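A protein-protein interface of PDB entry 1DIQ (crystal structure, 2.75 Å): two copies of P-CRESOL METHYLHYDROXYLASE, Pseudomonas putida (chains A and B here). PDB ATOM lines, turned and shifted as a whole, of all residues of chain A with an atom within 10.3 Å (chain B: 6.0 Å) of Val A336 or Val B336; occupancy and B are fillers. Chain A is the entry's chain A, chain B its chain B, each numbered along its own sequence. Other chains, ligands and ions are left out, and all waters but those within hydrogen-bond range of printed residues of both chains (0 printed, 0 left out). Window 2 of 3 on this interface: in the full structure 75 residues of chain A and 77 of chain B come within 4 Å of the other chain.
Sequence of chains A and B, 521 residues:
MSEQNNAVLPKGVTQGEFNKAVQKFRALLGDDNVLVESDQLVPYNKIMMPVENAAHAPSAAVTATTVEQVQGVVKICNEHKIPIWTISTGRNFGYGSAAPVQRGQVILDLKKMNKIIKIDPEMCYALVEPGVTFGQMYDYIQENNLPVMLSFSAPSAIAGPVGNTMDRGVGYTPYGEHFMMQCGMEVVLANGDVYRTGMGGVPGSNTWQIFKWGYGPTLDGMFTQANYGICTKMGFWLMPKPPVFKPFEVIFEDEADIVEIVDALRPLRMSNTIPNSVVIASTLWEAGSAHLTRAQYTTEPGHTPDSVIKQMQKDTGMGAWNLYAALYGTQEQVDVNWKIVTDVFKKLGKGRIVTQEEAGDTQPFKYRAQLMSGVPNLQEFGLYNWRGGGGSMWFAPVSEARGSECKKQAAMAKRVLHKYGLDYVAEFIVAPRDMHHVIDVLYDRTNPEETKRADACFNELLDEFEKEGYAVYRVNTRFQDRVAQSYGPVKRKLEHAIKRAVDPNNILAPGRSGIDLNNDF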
ATOM      1  N   VAL A 244      -6.702   3.751  30.405  1.00  0.00           N
ATOM      2  CA  VAL A 244      -6.345   5.097  29.944  1.00  0.00           C
ATOM      3  C   VAL A 244      -7.552   5.878  29.401  1.00  0.00           C
ATOM      4  O   VAL A 244      -8.426   5.323  28.735  1.00  0.00           O
ATOM      5  CB  VAL A 244      -5.026   5.152  29.002  1.00  0.00           C
ATOM      6  CG1 VAL A 244      -4.591   3.804  28.593  1.00  0.00           C
ATOM      7  CG2 VAL A 244      -5.183   6.049  27.753  1.00  0.00           C
ATOM      8  N   LYS A 246      -8.330   9.560  27.434  1.00  0.00           N
ATOM      9  CA  LYS A 246      -7.727  10.640  26.652  1.00  0.00           C
ATOM     10  C   LYS A 246      -8.735  11.693  26.168  1.00  0.00           C
ATOM     11  O   LYS A 246      -9.377  11.509  25.120  1.00  0.00           O
ATOM     12  CB  LYS A 246      -6.969  10.076  25.449  1.00  0.00           C
ATOM     13  CG  LYS A 246      -5.847  10.969  24.966  1.00  0.00           C
ATOM     14  CD  LYS A 246      -5.764  11.055  23.447  1.00  0.00           C
ATOM     15  CE  LYS A 246      -4.634  11.997  23.006  1.00  0.00           C
ATOM     16  NZ  LYS A 246      -3.288  11.400  23.181  1.00  0.00           N
ATOM     17  N   LEU A 268     -17.668   8.623  13.011  1.00  0.00           N
ATOM     18  CA  LEU A 268     -16.828   8.311  14.168  1.00  0.00           C
ATOM     19  C   LEU A 268     -17.653   7.930  15.388  1.00  0.00           C
ATOM     20  O   LEU A 268     -17.198   7.152  16.216  1.00  0.00           O
ATOM     21  CB  LEU A 268     -15.897   9.483  14.501  1.00  0.00           C
ATOM     22  CG  LEU A 268     -14.865   9.895  13.444  1.00  0.00           C
ATOM     23  CD1 LEU A 268     -14.123  11.126  13.918  1.00  0.00           C
ATOM     24  CD2 LEU A 268     -13.893   8.753  13.164  1.00  0.00           C
ATOM     25  N   ASN A 272     -18.349   3.903  16.764  1.00  0.00           N
ATOM     26  CA  ASN A 272     -17.929   3.883  18.164  1.00  0.00           C
ATOM     27  C   ASN A 272     -16.439   4.181  18.415  1.00  0.00           C
ATOM     28  O   ASN A 272     -15.894   3.841  19.475  1.00  0.00           O
ATOM     29  CB  ASN A 272     -18.384   2.579  18.849  1.00  0.00           C
ATOM     30  CG  ASN A 272     -18.846   2.803  20.263  1.00  0.00           C
ATOM     31  OD1 ASN A 272     -19.700   3.662  20.516  1.00  0.00           O
ATOM     32  ND2 ASN A 272     -18.274   2.049  21.206  1.00  0.00           N
ATOM     33  N   THR A 273     -15.794   4.833  17.438  1.00  0.00           N
ATOM     34  CA  THR A 273     -14.380   5.247  17.527  1.00  0.00           C
ATOM     35  C   THR A 273     -14.323   6.291  18.665  1.00  0.00           C
ATOM     36  O   THR A 273     -13.485   6.175  19.570  1.00  0.00           O
ATOM     37  CB  THR A 273     -13.872   5.790  16.164  1.00  0.00           C
ATOM     38  OG1 THR A 273     -14.056   4.774  15.168  1.00  0.00           O
ATOM     39  CG2 THR A 273     -12.375   6.163  16.233  1.00  0.00           C
ATOM     40  N   ILE A 274     -15.225   7.280  18.607  1.00  0.00           N
ATOM     41  CA  ILE A 274     -15.409   8.245  19.698  1.00  0.00           C
ATOM     42  C   ILE A 274     -16.690   7.624  20.318  1.00  0.00           C
ATOM     43  O   ILE A 274     -17.785   7.759  19.766  1.00  0.00           O
ATOM     44  CB  ILE A 274     -15.674   9.678  19.216  1.00  0.00           C
ATOM     45  CG1 ILE A 274     -14.447  10.225  18.485  1.00  0.00           C
ATOM     46  CG2 ILE A 274     -15.979  10.545  20.418  1.00  0.00           C
ATOM     47  CD1 ILE A 274     -14.658  11.579  17.809  1.00  0.00           C
ATOM     48  N   LEU A 327     -11.538   9.553  24.319  1.00  0.00           N
ATOM     49  CA  LEU A 327     -11.154   8.191  23.943  1.00  0.00           C
ATOM     50  C   LEU A 327     -10.904   7.386  25.209  1.00  0.00           C
ATOM     51  O   LEU A 327     -10.372   7.914  26.192  1.00  0.00           O
ATOM     52  CB  LEU A 327      -9.890   8.220  23.086  1.00  0.00           C
ATOM     53  CG  LEU A 327      -9.993   8.277  21.557  1.00  0.00           C
ATOM     54  CD1 LEU A 327     -11.158   9.100  21.000  1.00  0.00           C
ATOM     55  CD2 LEU A 327      -8.690   8.826  21.080  1.00  0.00           C
ATOM     56  N   TYR A 328     -11.398   6.145  25.215  1.00  0.00           N
ATOM     57  CA  TYR A 328     -11.274   5.235  26.370  1.00  0.00           C
ATOM     58  C   TYR A 328     -10.723   3.903  25.882  1.00  0.00           C
ATOM     59  O   TYR A 328     -10.862   3.569  24.708  1.00  0.00           O
ATOM     60  CB  TYR A 328     -12.656   4.984  27.039  1.00  0.00           C
ATOM     61  CG  TYR A 328     -13.489   6.227  27.347  1.00  0.00           C
ATOM     62  CD1 TYR A 328     -13.635   6.703  28.661  1.00  0.00           C
ATOM     63  CD2 TYR A 328     -14.108   6.951  26.311  1.00  0.00           C
ATOM     64  CE1 TYR A 328     -14.391   7.880  28.926  1.00  0.00           C
ATOM     65  CE2 TYR A 328     -14.840   8.118  26.560  1.00  0.00           C
ATOM     66  CZ  TYR A 328     -14.987   8.578  27.865  1.00  0.00           C
ATOM     67  OH  TYR A 328     -15.746   9.710  28.083  1.00  0.00           O
ATOM     68  N   GLY A 329     -10.087   3.159  26.778  1.00  0.00           N
ATOM     69  CA  GLY A 329      -9.547   1.860  26.427  1.00  0.00           C
ATOM     70  C   GLY A 329      -8.136   1.652  26.930  1.00  0.00           C
ATOM     71  O   GLY A 329      -7.714   2.290  27.912  1.00  0.00           O
ATOM     72  N   THR A 330      -7.433   0.705  26.295  1.00  0.00           N
ATOM     73  CA  THR A 330      -6.027   0.398  26.606  1.00  0.00           C
ATOM     74  C   THR A 330      -5.191   1.406  25.815  1.00  0.00           C
ATOM     75  O   THR A 330      -5.707   2.026  24.874  1.00  0.00           O
ATOM     76  CB  THR A 330      -5.612  -1.051  26.196  1.00  0.00           C
ATOM     77  OG1 THR A 330      -5.848  -1.257  24.795  1.00  0.00           O
ATOM     78  CG2 THR A 330      -6.348  -2.094  27.024  1.00  0.00           C
ATOM     79  N   GLN A 331      -3.913   1.554  26.172  1.00  0.00           N
ATOM     80  CA  GLN A 331      -3.033   2.502  25.493  1.00  0.00           C
ATOM     81  C   GLN A 331      -2.971   2.294  23.992  1.00  0.00           C
ATOM     82  O   GLN A 331      -3.140   3.247  23.236  1.00  0.00           O
ATOM     83  CB  GLN A 331      -1.633   2.487  26.119  1.00  0.00           C
ATOM     84  CG  GLN A 331      -0.731   3.672  25.719  1.00  0.00           C
ATOM     85  CD  GLN A 331      -1.300   5.028  26.105  1.00  0.00           C
ATOM     86  OE1 GLN A 331      -1.329   5.388  27.289  1.00  0.00           O
ATOM     87  NE2 GLN A 331      -1.747   5.790  25.105  1.00  0.00           N
ATOM     88  N   GLU A 332      -2.904   1.027  23.584  1.00  0.00           N
ATOM     89  CA  GLU A 332      -2.833   0.653  22.170  1.00  0.00           C
ATOM     90  C   GLU A 332      -4.149   0.933  21.452  1.00  0.00           C
ATOM     91  O   GLU A 332      -4.135   1.360  20.294  1.00  0.00           O
ATOM     92  CB  GLU A 332      -2.411  -0.811  22.001  1.00  0.00           C
ATOM     93  CG  GLU A 332      -1.074  -1.188  22.667  1.00  0.00           C
ATOM     94  CD  GLU A 332      -1.172  -1.380  24.187  1.00  0.00           C
ATOM     95  OE1 GLU A 332      -0.174  -1.093  24.889  1.00  0.00           O
ATOM     96  OE2 GLU A 332      -2.241  -1.819  24.681  1.00  0.00           O
ATOM     97  N   GLN A 333      -5.269   0.764  22.174  1.00  0.00           N
ATOM     98  CA  GLN A 333      -6.619   1.019  21.638  1.00  0.00           C
ATOM     99  C   GLN A 333      -6.817   2.521  21.400  1.00  0.00           C
ATOM    100  O   GLN A 333      -7.299   2.942  20.338  1.00  0.00           O
ATOM    101  CB  GLN A 333      -7.693   0.498  22.597  1.00  0.00           C
ATOM    102  CG  GLN A 333      -8.266  -0.859  22.236  1.00  0.00           C
ATOM    103  CD  GLN A 333      -9.098  -1.484  23.357  1.00  0.00           C
ATOM    104  OE1 GLN A 333      -9.119  -1.007  24.497  1.00  0.00           O
ATOM    105  NE2 GLN A 333      -9.761  -2.589  23.038  1.00  0.00           N
ATOM    106  N   VAL A 334      -6.374   3.312  22.375  1.00  0.00           N
ATOM    107  CA  VAL A 334      -6.443   4.772  22.333  1.00  0.00           C
ATOM    108  C   VAL A 334      -5.521   5.343  21.246  1.00  0.00           C
ATOM    109  O   VAL A 334      -5.920   6.266  20.525  1.00  0.00           O
ATOM    110  CB  VAL A 334      -6.093   5.378  23.733  1.00  0.00           C
ATOM    111  CG1 VAL A 334      -5.994   6.913  23.694  1.00  0.00           C
ATOM    112  CG2 VAL A 334      -7.149   4.951  24.749  1.00  0.00           C
ATOM    113  N   ASP A 335      -4.330   4.752  21.090  1.00  0.00           N
ATOM    114  CA  ASP A 335      -3.368   5.210  20.079  1.00  0.00           C
ATOM    115  C   ASP A 335      -3.846   5.039  18.626  1.00  0.00           C
ATOM    116  O   ASP A 335      -3.660   5.945  17.800  1.00  0.00           O
ATOM    117  CB  ASP A 335      -1.980   4.581  20.287  1.00  0.00           C
ATOM    118  CG  ASP A 335      -1.256   5.116  21.533  1.00  0.00           C
ATOM    119  OD1 ASP A 335      -1.504   6.277  21.948  1.00  0.00           O
ATOM    120  OD2 ASP A 335      -0.428   4.366  22.109  1.00  0.00           O
ATOM    121  N   VAL A 336      -4.541   3.937  18.331  1.00  0.00           N
ATOM    122  CA  VAL A 336      -5.027   3.723  16.966  1.00  0.00           C
ATOM    123  C   VAL A 336      -6.257   4.562  16.683  1.00  0.00           C
ATOM    124  O   VAL A 336      -6.461   4.998  15.547  1.00  0.00           O
ATOM    125  CB  VAL A 336      -5.265   2.209  16.583  1.00  0.00           C
ATOM    126  CG1 VAL A 336      -4.158   1.347  17.127  1.00  0.00           C
ATOM    127  CG2 VAL A 336      -6.616   1.698  17.018  1.00  0.00           C
ATOM    128  N   ASN A 337      -7.048   4.807  17.733  1.00  0.00           N
ATOM    129  CA  ASN A 337      -8.255   5.613  17.623  1.00  0.00           C
ATOM    130  C   ASN A 337      -7.894   7.079  17.506  1.00  0.00           C
ATOM    131  O   ASN A 337      -8.563   7.816  16.771  1.00  0.00           O
ATOM    132  CB  ASN A 337      -9.199   5.368  18.799  1.00  0.00           C
ATOM    133  CG  ASN A 337     -10.060   4.116  18.623  1.00  0.00           C
ATOM    134  OD1 ASN A 337     -10.059   3.471  17.566  1.00  0.00           O
ATOM    135  ND2 ASN A 337     -10.814   3.781  19.659  1.00  0.00           N
ATOM    136  N   TRP A 338      -6.783   7.469  18.151  1.00  0.00           N
ATOM    137  CA  TRP A 338      -6.288   8.849  18.080  1.00  0.00           C
ATOM    138  C   TRP A 338      -5.768   9.157  16.684  1.00  0.00           C
ATOM    139  O   TRP A 338      -6.006  10.243  16.164  1.00  0.00           O
ATOM    140  CB  TRP A 338      -5.221   9.142  19.145  1.00  0.00           C
ATOM    141  CG  TRP A 338      -4.729  10.598  19.174  1.00  0.00           C
ATOM    142  CD1 TRP A 338      -3.466  11.030  18.891  1.00  0.00           C
ATOM    143  CD2 TRP A 338      -5.499  11.782  19.449  1.00  0.00           C
ATOM    144  NE1 TRP A 338      -3.394  12.399  18.960  1.00  0.00           N
ATOM    145  CE2 TRP A 338      -4.620  12.893  19.302  1.00  0.00           C
ATOM    146  CE3 TRP A 338      -6.849  12.022  19.804  1.00  0.00           C
ATOM    147  CZ2 TRP A 338      -5.040  14.228  19.498  1.00  0.00           C
ATOM    148  CZ3 TRP A 338      -7.272  13.357  19.998  1.00  0.00           C
ATOM    149  CH2 TRP A 338      -6.364  14.441  19.843  1.00  0.00           C
ATOM    150  N   LYS A 339      -5.145   8.158  16.059  1.00  0.00           N
ATOM    151  CA  LYS A 339      -4.620   8.282  14.706  1.00  0.00           C
ATOM    152  C   LYS A 339      -5.792   8.440  13.702  1.00  0.00           C
ATOM    153  O   LYS A 339      -5.696   9.238  12.768  1.00  0.00           O
ATOM    154  CB  LYS A 339      -3.724   7.072  14.392  1.00  0.00           C
ATOM    155  CG  LYS A 339      -2.460   7.375  13.578  1.00  0.00           C
ATOM    156  CD  LYS A 339      -2.691   7.202  12.068  1.00  0.00           C
ATOM    157  CE  LYS A 339      -1.524   7.733  11.241  1.00  0.00           C
ATOM    158  NZ  LYS A 339      -1.822   7.733   9.777  1.00  0.00           N
ATOM    159  N   ILE A 340      -6.919   7.767  13.965  1.00  0.00           N
ATOM    160  CA  ILE A 340      -8.124   7.837  13.108  1.00  0.00           C
ATOM    161  C   ILE A 340      -8.822   9.194  13.228  1.00  0.00           C
ATOM    162  O   ILE A 340      -9.177   9.798  12.208  1.00  0.00           O
ATOM    163  CB  ILE A 340      -9.141   6.681  13.426  1.00  0.00           C
ATOM    164  CG1 ILE A 340      -8.528   5.338  13.035  1.00  0.00           C
ATOM    165  CG2 ILE A 340     -10.493   6.868  12.673  1.00  0.00           C
ATOM    166  CD1 ILE A 340      -9.235   4.168  13.616  1.00  0.00           C
ATOM    167  N   VAL A 341      -8.980   9.665  14.470  1.00  0.00           N
ATOM    168  CA  VAL A 341      -9.632  10.951  14.769  1.00  0.00           C
ATOM    169  C   VAL A 341      -8.830  12.143  14.206  1.00  0.00           C
ATOM    170  O   VAL A 341      -9.407  13.026  13.546  1.00  0.00           O
ATOM    171  CB  VAL A 341      -9.904  11.104  16.314  1.00  0.00           C
ATOM    172  CG1 VAL A 341     -10.487  12.467  16.642  1.00  0.00           C
ATOM    173  CG2 VAL A 341     -10.888  10.045  16.778  1.00  0.00           C
ATOM    174  N   THR A 342      -7.506  12.106  14.417  1.00  0.00           N
ATOM    175  CA  THR A 342      -6.550  13.121  13.958  1.00  0.00           C
ATOM    176  C   THR A 342      -6.558  13.276  12.434  1.00  0.00           C
ATOM    177  O   THR A 342      -6.606  14.407  11.931  1.00  0.00           O
ATOM    178  CB  THR A 342      -5.137  12.802  14.522  1.00  0.00           C
ATOM    179  OG1 THR A 342      -4.999  13.456  15.790  1.00  0.00           O
ATOM    180  CG2 THR A 342      -3.976  13.206  13.589  1.00  0.00           C
ATOM    181  N   ASP A 343      -6.580  12.148  11.716  1.00  0.00           N
ATOM    182  CA  ASP A 343      -6.603  12.154  10.255  1.00  0.00           C
ATOM    183  C   ASP A 343      -7.881  12.739   9.685  1.00  0.00           C
ATOM    184  O   ASP A 343      -7.817  13.472   8.707  1.00  0.00           O
ATOM    185  CB  ASP A 343      -6.345  10.758   9.685  1.00  0.00           C
ATOM    186  CG  ASP A 343      -4.884  10.302   9.861  1.00  0.00           C
ATOM    187  OD1 ASP A 343      -4.612   9.100   9.637  1.00  0.00           O
ATOM    188  OD2 ASP A 343      -4.004  11.125  10.226  1.00  0.00           O
ATOM    189  N   VAL A 344      -9.014  12.500  10.354  1.00  0.00           N
ATOM    190  CA  VAL A 344     -10.328  13.018   9.928  1.00  0.00           C
ATOM    191  C   VAL A 344     -10.330  14.546   9.996  1.00  0.00           C
ATOM    192  O   VAL A 344     -10.749  15.205   9.042  1.00  0.00           O
ATOM    193  CB  VAL A 344     -11.523  12.398  10.771  1.00  0.00           C
ATOM    194  CG1 VAL A 344     -12.866  13.098  10.470  1.00  0.00           C
ATOM    195  CG2 VAL A 344     -11.687  10.925  10.438  1.00  0.00           C
ATOM    196  N   THR B 330     -11.525  -1.080  11.566  1.00  0.00           N
ATOM    197  CA  THR B 330     -10.449  -0.864  10.578  1.00  0.00           C
ATOM    198  C   THR B 330      -9.397  -1.917  10.867  1.00  0.00           C
ATOM    199  O   THR B 330      -9.410  -2.504  11.955  1.00  0.00           O
ATOM    200  CB  THR B 330      -9.796   0.551  10.686  1.00  0.00           C
ATOM    201  OG1 THR B 330      -9.258   0.747  12.004  1.00  0.00           O
ATOM    202  CG2 THR B 330     -10.811   1.663  10.336  1.00  0.00           C
ATOM    203  N   GLN B 331      -8.483  -2.144   9.920  1.00  0.00           N
ATOM    204  CA  GLN B 331      -7.436  -3.159  10.074  1.00  0.00           C
ATOM    205  C   GLN B 331      -6.602  -2.987  11.321  1.00  0.00           C
ATOM    206  O   GLN B 331      -6.393  -3.954  12.055  1.00  0.00           O
ATOM    207  CB  GLN B 331      -6.550  -3.231   8.827  1.00  0.00           C
ATOM    208  CG  GLN B 331      -5.653  -4.481   8.739  1.00  0.00           C
ATOM    209  CD  GLN B 331      -6.440  -5.796   8.727  1.00  0.00           C
ATOM    210  OE1 GLN B 331      -7.066  -6.156   7.724  1.00  0.00           O
ATOM    211  NE2 GLN B 331      -6.404  -6.520   9.852  1.00  0.00           N
ATOM    212  N   GLU B 332      -6.274  -1.731  11.624  1.00  0.00           N
ATOM    213  CA  GLU B 332      -5.468  -1.379  12.794  1.00  0.00           C
ATOM    214  C   GLU B 332      -6.254  -1.572  14.090  1.00  0.00           C
ATOM    215  O   GLU B 332      -5.678  -2.009  15.094  1.00  0.00           O
ATOM    216  CB  GLU B 332      -4.932   0.057  12.686  1.00  0.00           C
ATOM    217  CG  GLU B 332      -4.093   0.360  11.426  1.00  0.00           C
ATOM    218  CD  GLU B 332      -4.935   0.584  10.161  1.00  0.00           C
ATOM    219  OE1 GLU B 332      -4.448   0.238   9.060  1.00  0.00           O
ATOM    220  OE2 GLU B 332      -6.074   1.106  10.265  1.00  0.00           O
ATOM    221  N   GLN B 333      -7.571  -1.308  14.038  1.00  0.00           N
ATOM    222  CA  GLN B 333      -8.480  -1.484  15.189  1.00  0.00           C
ATOM    223  C   GLN B 333      -8.621  -2.973  15.531  1.00  0.00           C
ATOM    224  O   GLN B 333      -8.501  -3.364  16.698  1.00  0.00           O
ATOM    225  CB  GLN B 333      -9.859  -0.889  14.892  1.00  0.00           C
ATOM    226  CG  GLN B 333     -10.067   0.509  15.428  1.00  0.00           C
ATOM    227  CD  GLN B 333     -11.323   1.190  14.887  1.00  0.00           C
ATOM    228  OE1 GLN B 333     -11.978   0.699  13.961  1.00  0.00           O
ATOM    229  NE2 GLN B 333     -11.646   2.356  15.453  1.00  0.00           N
ATOM    230  N   VAL B 334      -8.788  -3.790  14.484  1.00  0.00           N
ATOM    231  CA  VAL B 334      -8.925  -5.246  14.579  1.00  0.00           C
ATOM    232  C   VAL B 334      -7.619  -5.896  15.060  1.00  0.00           C
ATOM    233  O   VAL B 334      -7.660  -6.798  15.900  1.00  0.00           O
ATOM    234  CB  VAL B 334      -9.376  -5.840  13.208  1.00  0.00           C
ATOM    235  CG1 VAL B 334      -9.392  -7.370  13.223  1.00  0.00           C
ATOM    236  CG2 VAL B 334     -10.757  -5.311  12.850  1.00  0.00           C
ATOM    237  N   ASP B 335      -6.475  -5.406  14.568  1.00  0.00           N
ATOM    238  CA  ASP B 335      -5.171  -5.937  14.963  1.00  0.00           C
ATOM    239  C   ASP B 335      -4.832  -5.745  16.444  1.00  0.00           C
ATOM    240  O   ASP B 335      -4.287  -6.671  17.057  1.00  0.00           O
ATOM    241  CB  ASP B 335      -4.047  -5.385  14.074  1.00  0.00           C
ATOM    242  CG  ASP B 335      -4.090  -5.935  12.636  1.00  0.00           C
ATOM    243  OD1 ASP B 335      -4.586  -7.066  12.418  1.00  0.00           O
ATOM    244  OD2 ASP B 335      -3.627  -5.219  11.714  1.00  0.00           O
ATOM    245  N   VAL B 336      -5.203  -4.595  17.036  1.00  0.00           N
ATOM    246  CA  VAL B 336      -4.914  -4.360  18.461  1.00  0.00           C
ATOM    247  C   VAL B 336      -5.878  -5.124  19.349  1.00  0.00           C
ATOM    248  O   VAL B 336      -5.491  -5.590  20.429  1.00  0.00           O
ATOM    249  CB  VAL B 336      -4.826  -2.839  18.887  1.00  0.00           C
ATOM    250  CG1 VAL B 336      -4.112  -2.050  17.845  1.00  0.00           C
ATOM    251  CG2 VAL B 336      -6.171  -2.223  19.194  1.00  0.00           C
ATOM    252  N   ASN B 337      -7.110  -5.297  18.857  1.00  0.00           N
ATOM    253  CA  ASN B 337      -8.137  -6.023  19.595  1.00  0.00           C
ATOM    254  C   ASN B 337      -7.844  -7.514  19.551  1.00  0.00           C
ATOM    255  O   ASN B 337      -8.070  -8.215  20.540  1.00  0.00           O
ATOM    256  CB  ASN B 337      -9.540  -5.711  19.062  1.00  0.00           C
ATOM    257  CG  ASN B 337     -10.102  -4.396  19.597  1.00  0.00           C
ATOM    258  OD1 ASN B 337      -9.520  -3.751  20.470  1.00  0.00           O
ATOM    259  ND2 ASN B 337     -11.249  -4.001  19.071  1.00  0.00           N
ATOM    260  N   TRP B 338      -7.261  -7.970  18.433  1.00  0.00           N
ATOM    261  CA  TRP B 338      -6.886  -9.379  18.270  1.00  0.00           C
ATOM    262  C   TRP B 338      -5.749  -9.733  19.219  1.00  0.00           C
ATOM    263  O   TRP B 338      -5.754 -10.805  19.805  1.00  0.00           O
ATOM    264  CB  TRP B 338      -6.521  -9.722  16.809  1.00  0.00           C
ATOM    265  CG  TRP B 338      -6.200 -11.198  16.564  1.00  0.00           C
ATOM    266  CD1 TRP B 338      -4.993 -11.711  16.191  1.00  0.00           C
ATOM    267  CD2 TRP B 338      -7.077 -12.332  16.732  1.00  0.00           C
ATOM    268  NE1 TRP B 338      -5.049 -13.080  16.124  1.00  0.00           N
ATOM    269  CE2 TRP B 338      -6.311 -13.494  16.448  1.00  0.00           C
ATOM    270  CE3 TRP B 338      -8.437 -12.482  17.094  1.00  0.00           C
ATOM    271  CZ2 TRP B 338      -6.858 -14.799  16.516  1.00  0.00           C
ATOM    272  CZ3 TRP B 338      -8.980 -13.770  17.163  1.00  0.00           C
ATOM    273  CH2 TRP B 338      -8.188 -14.915  16.873  1.00  0.00           C
ATOM    274  N   LYS B 339      -4.838  -8.786  19.425  1.00  0.00           N
ATOM    275  CA  LYS B 339      -3.709  -8.963  20.322  1.00  0.00           C
ATOM    276  C   LYS B 339      -4.217  -9.050  21.789  1.00  0.00           C
ATOM    277  O   LYS B 339      -3.705  -9.854  22.575  1.00  0.00           O
ATOM    278  CB  LYS B 339      -2.700  -7.817  20.107  1.00  0.00           C
ATOM    279  CG  LYS B 339      -1.210  -8.211  20.169  1.00  0.00           C
ATOM    280  CD  LYS B 339      -0.642  -8.035  21.577  1.00  0.00           C
ATOM    281  CE  LYS B 339       0.743  -8.656  21.713  1.00  0.00           C
ATOM    282  NZ  LYS B 339       1.241  -8.638  23.128  1.00  0.00           N
ATOM    283  N   ILE B 340      -5.273  -8.291  22.118  1.00  0.00           N
ATOM    284  CA  ILE B 340      -5.873  -8.295  23.467  1.00  0.00           C
ATOM    285  C   ILE B 340      -6.631  -9.598  23.729  1.00  0.00           C
ATOM    286  O   ILE B 340      -6.484 -10.183  24.802  1.00  0.00           O
ATOM    287  CB  ILE B 340      -6.834  -7.090  23.676  1.00  0.00           C
ATOM    288  CG1 ILE B 340      -6.044  -5.793  23.651  1.00  0.00           C
ATOM    289  CG2 ILE B 340      -7.614  -7.202  25.009  1.00  0.00           C
ATOM    290  CD1 ILE B 340      -6.908  -4.574  23.509  1.00  0.00           C
ATOM    291  N   VAL B 341      -7.415 -10.048  22.744  1.00  0.00           N
ATOM    292  CA  VAL B 341      -8.211 -11.286  22.845  1.00  0.00           C
ATOM    293  C   VAL B 341      -7.307 -12.533  22.953  1.00  0.00           C
ATOM    294  O   VAL B 341      -7.507 -13.376  23.840  1.00  0.00           O
ATOM    295  CB  VAL B 341      -9.232 -11.409  21.650  1.00  0.00           C
ATOM    296  CG1 VAL B 341      -9.963 -12.726  21.689  1.00  0.00           C
ATOM    297  CG2 VAL B 341     -10.243 -10.291  21.710  1.00  0.00           C
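The side-chain amide nitrogen of Gln B333 sits at hydrogen-bond distance from the side-chain hydroxyl of Thr A273, at 3.4 Å. The side-chain amide oxygen of Asn B337 is in hydrogen-bond range of the side-chain amide nitrogen of Gln A333 (2.8 Å). The side-chain amide nitrogen (NE2) of Gln B333 is in hydrogen-bond range of the side-chain amide oxygen (OD1) of Asn A337 (2.9 Å).
O of Leu A268 lies within hydrogen-bond range of N of Thr A273 (3.0 Å). OE1 of Gln A333 is in hydrogen-bond range of N of Thr A330 (3.0 Å). The backbone NH of Thr B330 lies within hydrogen-bond range of the side-chain amide oxygen of Gln B333, 3.0 Å away.
Among the printed residues, pairs that only touch across the chains: Thr A330 with Ile B340 (3.7 Å), Gln A333 with Val B336 (3.9 Å), Gln A333 with Ile B340 (3.5 Å), Val A336 with Gln B333 (3.98 Å), Val A336 with Val B336 (3.5 Å), Ile A340 with Thr B330 (3.8 Å) and Ile A340 with Gln B333 (3.5 Å).
Of the printed residues of chain B, Gln A333 touches Val B336 (3.9 Å), Asn B337 (2.8 Å) and Ile B340 (3.5 Å). Of the printed residues of chain B, Val A336 touches Gln B333 (3.98 Å) and Val B336 (3.5 Å). Printed residues of chain B within 4 Å of Ile A340: Thr B330 and Gln B333. No residue of chain A comes within 4 Å of Asp B335. Of chain A, only Gln A333 and Val A336 come within 4 Å of Val B336. Asn B337 touches one residue of chain A. The nearest printed residue of chain B that does not touch Ile A340 is Glu B332 (5.5 Å).
Hydrophobic or aromatic side chains of chain B that line the printed part of chain A: Val B336 and Ile B340. Of the 24 printed residues of chain A, 6 touch a printed residue of chain B. Printed residues of chain A that touch a printed residue of chain B: Thr A273, Thr A330, Gln A333, Val A336, Asn A337 and Ile A340. Hydrophobic or aromatic side chains of chain A within 4 Å of the printed part of chain B: Val A336 and Ile A340. Along chain A the printed residues that touch a printed residue of chain B span positions 273 to 340. Among the printed residues, no Asp or Glu carboxylate lies within 4 Å of a Lys or Arg side-chain nitrogen of the other chain.
Thr A330 touches Ile B340, and with the chains exchanged Ile A340 touches Thr B330. Gln A333 touches Val B336, and with the chains exchanged Val A336 touches Gln B333. Gln A333 touches Asn B337, and with the chains exchanged Asn A337 touches Gln B333. Gln A333 touches Ile B340, and with the chains exchanged Ile A340 touches Gln B333. Of the 10 pairs that touch across the chains among the printed residues, 9 have their exchanged pair printed and touching as well.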
